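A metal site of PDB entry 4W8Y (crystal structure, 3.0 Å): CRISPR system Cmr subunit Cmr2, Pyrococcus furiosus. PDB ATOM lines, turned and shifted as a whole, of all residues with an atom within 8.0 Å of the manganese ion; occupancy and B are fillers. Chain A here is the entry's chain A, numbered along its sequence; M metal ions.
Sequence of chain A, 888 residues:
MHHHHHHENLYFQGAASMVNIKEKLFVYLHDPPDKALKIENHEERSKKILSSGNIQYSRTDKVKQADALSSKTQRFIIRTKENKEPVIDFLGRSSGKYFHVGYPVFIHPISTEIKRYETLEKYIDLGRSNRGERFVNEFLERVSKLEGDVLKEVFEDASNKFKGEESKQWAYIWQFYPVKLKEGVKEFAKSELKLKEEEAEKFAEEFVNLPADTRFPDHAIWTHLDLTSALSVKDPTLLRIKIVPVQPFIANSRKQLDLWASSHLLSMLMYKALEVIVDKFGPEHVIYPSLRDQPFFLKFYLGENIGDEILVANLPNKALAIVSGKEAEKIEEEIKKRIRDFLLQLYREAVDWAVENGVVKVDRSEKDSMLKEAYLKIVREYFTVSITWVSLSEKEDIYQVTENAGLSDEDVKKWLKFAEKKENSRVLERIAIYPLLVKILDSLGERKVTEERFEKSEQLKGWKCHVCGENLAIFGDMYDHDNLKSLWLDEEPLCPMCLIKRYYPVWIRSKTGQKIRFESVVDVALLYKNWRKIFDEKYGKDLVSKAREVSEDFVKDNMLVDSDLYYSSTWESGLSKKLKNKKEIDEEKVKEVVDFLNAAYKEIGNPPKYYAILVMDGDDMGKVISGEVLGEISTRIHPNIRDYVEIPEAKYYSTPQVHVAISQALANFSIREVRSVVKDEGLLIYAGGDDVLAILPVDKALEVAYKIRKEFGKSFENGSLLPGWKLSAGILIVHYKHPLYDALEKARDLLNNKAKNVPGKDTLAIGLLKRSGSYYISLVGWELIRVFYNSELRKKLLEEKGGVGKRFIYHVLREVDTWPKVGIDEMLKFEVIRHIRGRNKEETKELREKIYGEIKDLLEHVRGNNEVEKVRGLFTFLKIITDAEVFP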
ATOM      1  N   ARG A 672       6.266  24.750 -24.404  1.00  0.00           N
ATOM      2  CA  ARG A 672       5.719  25.995 -24.941  1.00  0.00           C
ATOM      3  C   ARG A 672       4.328  26.338 -24.410  1.00  0.00           C
ATOM      4  O   ARG A 672       4.112  27.423 -23.856  1.00  0.00           O
ATOM      5  CB  ARG A 672       5.680  25.912 -26.465  1.00  0.00           C
ATOM      6  CG  ARG A 672       6.103  27.189 -27.176  1.00  0.00           C
ATOM      7  CD  ARG A 672       6.074  27.017 -28.687  1.00  0.00           C
ATOM      8  NE  ARG A 672       6.680  25.749 -29.088  1.00  0.00           N
ATOM      9  CZ  ARG A 672       7.991  25.540 -29.216  1.00  0.00           C
ATOM     10  NH1 ARG A 672       8.838  26.534 -28.967  1.00  0.00           N
ATOM     11  NH2 ARG A 672       8.437  24.353 -29.575  1.00  0.00           N
ATOM     12  N   GLU A 673       3.381  25.411 -24.589  1.00  0.00           N
ATOM     13  CA  GLU A 673       1.976  25.726 -24.400  1.00  0.00           C
ATOM     14  C   GLU A 673       1.574  25.942 -22.941  1.00  0.00           C
ATOM     15  O   GLU A 673       0.911  26.925 -22.616  1.00  0.00           O
ATOM     16  CB  GLU A 673       1.117  24.632 -25.030  1.00  0.00           C
ATOM     17  CG  GLU A 673       1.296  24.508 -26.543  1.00  0.00           C
ATOM     18  CD  GLU A 673       1.215  25.842 -27.264  1.00  0.00           C
ATOM     19  OE1 GLU A 673       0.231  26.595 -27.048  1.00  0.00           O
ATOM     20  OE2 GLU A 673       2.136  26.155 -28.046  1.00  0.00           O
ATOM     21  N   VAL A 674       1.978  25.023 -22.071  1.00  0.00           N
ATOM     22  CA  VAL A 674       1.638  25.107 -20.659  1.00  0.00           C
ATOM     23  C   VAL A 674       2.191  26.394 -20.051  1.00  0.00           C
ATOM     24  O   VAL A 674       1.493  27.131 -19.367  1.00  0.00           O
ATOM     25  CB  VAL A 674       2.174  23.901 -19.874  1.00  0.00           C
ATOM     26  CG1 VAL A 674       1.703  23.950 -18.430  1.00  0.00           C
ATOM     27  CG2 VAL A 674       1.735  22.627 -20.525  1.00  0.00           C
ATOM     28  N   SER A 676       2.949  29.001 -21.621  1.00  0.00           N
ATOM     29  CA  SER A 676       2.258  30.135 -22.217  1.00  0.00           C
ATOM     30  C   SER A 676       0.937  30.408 -21.506  1.00  0.00           C
ATOM     31  O   SER A 676       0.551  31.554 -21.323  1.00  0.00           O
ATOM     32  CB  SER A 676       2.004  29.895 -23.717  1.00  0.00           C
ATOM     33  OG  SER A 676       1.035  28.884 -23.905  1.00  0.00           O
ATOM     34  N   VAL A 677       0.252  29.336 -21.106  1.00  0.00           N
ATOM     35  CA  VAL A 677      -1.006  29.459 -20.380  1.00  0.00           C
ATOM     36  C   VAL A 677      -0.810  30.028 -18.976  1.00  0.00           C
ATOM     37  O   VAL A 677      -1.516  30.954 -18.560  1.00  0.00           O
ATOM     38  CB  VAL A 677      -1.742  28.113 -20.269  1.00  0.00           C
ATOM     39  CG1 VAL A 677      -3.016  28.266 -19.453  1.00  0.00           C
ATOM     40  CG2 VAL A 677      -2.065  27.562 -21.647  1.00  0.00           C
ATOM     41  N   LYS A 707      -7.574  25.655 -19.829  1.00  0.00           N
ATOM     42  CA  LYS A 707      -6.853  26.081 -21.024  1.00  0.00           C
ATOM     43  C   LYS A 707      -5.668  25.175 -21.320  1.00  0.00           C
ATOM     44  O   LYS A 707      -5.328  24.940 -22.477  1.00  0.00           O
ATOM     45  CB  LYS A 707      -6.408  27.543 -20.890  1.00  0.00           C
ATOM     46  CG  LYS A 707      -7.554  28.526 -20.878  1.00  0.00           C
ATOM     47  CD  LYS A 707      -7.109  29.940 -21.194  1.00  0.00           C
ATOM     48  CE  LYS A 707      -8.287  30.906 -21.132  1.00  0.00           C
ATOM     49  NZ  LYS A 707      -7.908  32.294 -21.543  1.00  0.00           N
ATOM     50  N   GLU A 711      -5.359  23.142 -24.755  1.00  0.00           N
ATOM     51  CA  GLU A 711      -4.162  23.189 -25.589  1.00  0.00           C
ATOM     52  C   GLU A 711      -3.567  21.788 -25.733  1.00  0.00           C
ATOM     53  O   GLU A 711      -2.944  21.463 -26.738  1.00  0.00           O
ATOM     54  CB  GLU A 711      -3.138  24.142 -24.992  1.00  0.00           C
ATOM     55  CG  GLU A 711      -2.251  24.799 -26.034  1.00  0.00           C
ATOM     56  CD  GLU A 711      -2.801  26.121 -26.518  1.00  0.00           C
ATOM     57  OE1 GLU A 711      -3.496  26.797 -25.740  1.00  0.00           O
ATOM     58  OE2 GLU A 711      -2.529  26.478 -27.694  1.00  0.00           O
ATOM     59  N   LYS A 714      -5.560  20.198 -28.627  1.00  0.00           N
ATOM     60  CA  LYS A 714      -5.237  20.602 -29.991  1.00  0.00           C
ATOM     61  C   LYS A 714      -4.310  19.599 -30.666  1.00  0.00           C
ATOM     62  O   LYS A 714      -3.503  18.950 -30.007  1.00  0.00           O
ATOM     63  CB  LYS A 714      -4.607  21.995 -30.006  1.00  0.00           C
ATOM     64  CG  LYS A 714      -5.554  23.118 -29.601  1.00  0.00           C
ATOM     65  CD  LYS A 714      -4.901  24.469 -29.795  1.00  0.00           C
ATOM     66  CE  LYS A 714      -5.608  25.549 -28.989  1.00  0.00           C
ATOM     67  NZ  LYS A 714      -4.933  26.869 -29.150  1.00  0.00           N
ATOM     68  N   PHE A 716      -2.686  20.545 -33.765  1.00  0.00           N
ATOM     69  CA  PHE A 716      -1.675  21.332 -34.454  1.00  0.00           C
ATOM     70  C   PHE A 716      -1.631  22.783 -33.961  1.00  0.00           C
ATOM     71  O   PHE A 716      -2.670  23.418 -33.775  1.00  0.00           O
ATOM     72  CB  PHE A 716      -1.905  21.313 -35.963  1.00  0.00           C
ATOM     73  CG  PHE A 716      -1.997  19.929 -36.554  1.00  0.00           C
ATOM     74  CD1 PHE A 716      -0.851  19.244 -36.935  1.00  0.00           C
ATOM     75  CD2 PHE A 716      -3.220  19.309 -36.737  1.00  0.00           C
ATOM     76  CE1 PHE A 716      -0.927  17.980 -37.477  1.00  0.00           C
ATOM     77  CE2 PHE A 716      -3.304  18.050 -37.281  1.00  0.00           C
ATOM     78  CZ  PHE A 716      -2.164  17.377 -37.650  1.00  0.00           C
ATOM     79  N   GLU A 717      -0.413  23.280 -33.758  1.00  0.00           N
ATOM     80  CA  GLU A 717      -0.173  24.698 -33.555  1.00  0.00           C
ATOM     81  C   GLU A 717       0.898  25.101 -34.556  1.00  0.00           C
ATOM     82  O   GLU A 717       2.045  24.664 -34.454  1.00  0.00           O
ATOM     83  CB  GLU A 717       0.299  25.016 -32.132  1.00  0.00           C
ATOM     84  CG  GLU A 717       0.653  26.489 -31.928  1.00  0.00           C
ATOM     85  CD  GLU A 717      -0.364  27.249 -31.087  1.00  0.00           C
ATOM     86  OE1 GLU A 717      -0.331  28.500 -31.111  1.00  0.00           O
ATOM     87  OE2 GLU A 717      -1.192  26.610 -30.414  1.00  0.00           O
ATOM     88  N   ASN A 718       0.523  25.935 -35.526  1.00  0.00           N
ATOM     89  CA  ASN A 718       1.371  26.240 -36.665  1.00  0.00           C
ATOM     90  C   ASN A 718       1.791  24.955 -37.365  1.00  0.00           C
ATOM     91  O   ASN A 718       0.969  24.057 -37.580  1.00  0.00           O
ATOM     92  CB  ASN A 718       2.602  27.045 -36.243  1.00  0.00           C
ATOM     93  CG  ASN A 718       2.241  28.366 -35.589  1.00  0.00           C
ATOM     94  OD1 ASN A 718       1.082  28.798 -35.642  1.00  0.00           O
ATOM     95  ND2 ASN A 718       3.227  29.025 -34.997  1.00  0.00           N
ATOM     96  N   LEU A 722       0.919  18.796 -31.790  1.00  0.00           N
ATOM     97  CA  LEU A 722       0.537  18.805 -30.380  1.00  0.00           C
ATOM     98  C   LEU A 722      -0.086  17.454 -30.066  1.00  0.00           C
ATOM     99  O   LEU A 722      -0.445  16.717 -30.971  1.00  0.00           O
ATOM    100  CB  LEU A 722      -0.441  19.949 -30.079  1.00  0.00           C
ATOM    101  CG  LEU A 722       0.154  21.355 -29.895  1.00  0.00           C
ATOM    102  CD1 LEU A 722      -0.942  22.368 -29.595  1.00  0.00           C
ATOM    103  CD2 LEU A 722       1.194  21.355 -28.795  1.00  0.00           C
HETATM  104 MN    MN M   1      -0.948  27.650 -28.516  1.00  0.00          MN
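NZ of Lys 714 is in salt-bridge range of OE1 of Glu 711, 3.7 Å away. NZ of Lys 714 lies close to OE2 of Glu 717, at 3.96 Å.
Three residues have an atom within 4 Å of the manganese ion: Glu 673, Glu 711 and Glu 717.
The manganese ion is bound by OE2 of Glu 711 (2.1 Å), OE1 of Glu 673 (2.2 Å) and OE2 of Glu 717 (2.2 Å). The manganese ion has three donor atoms within binding distance. Slightly farther from the manganese ion lies OE1 of Glu 717 (2.8 Å).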
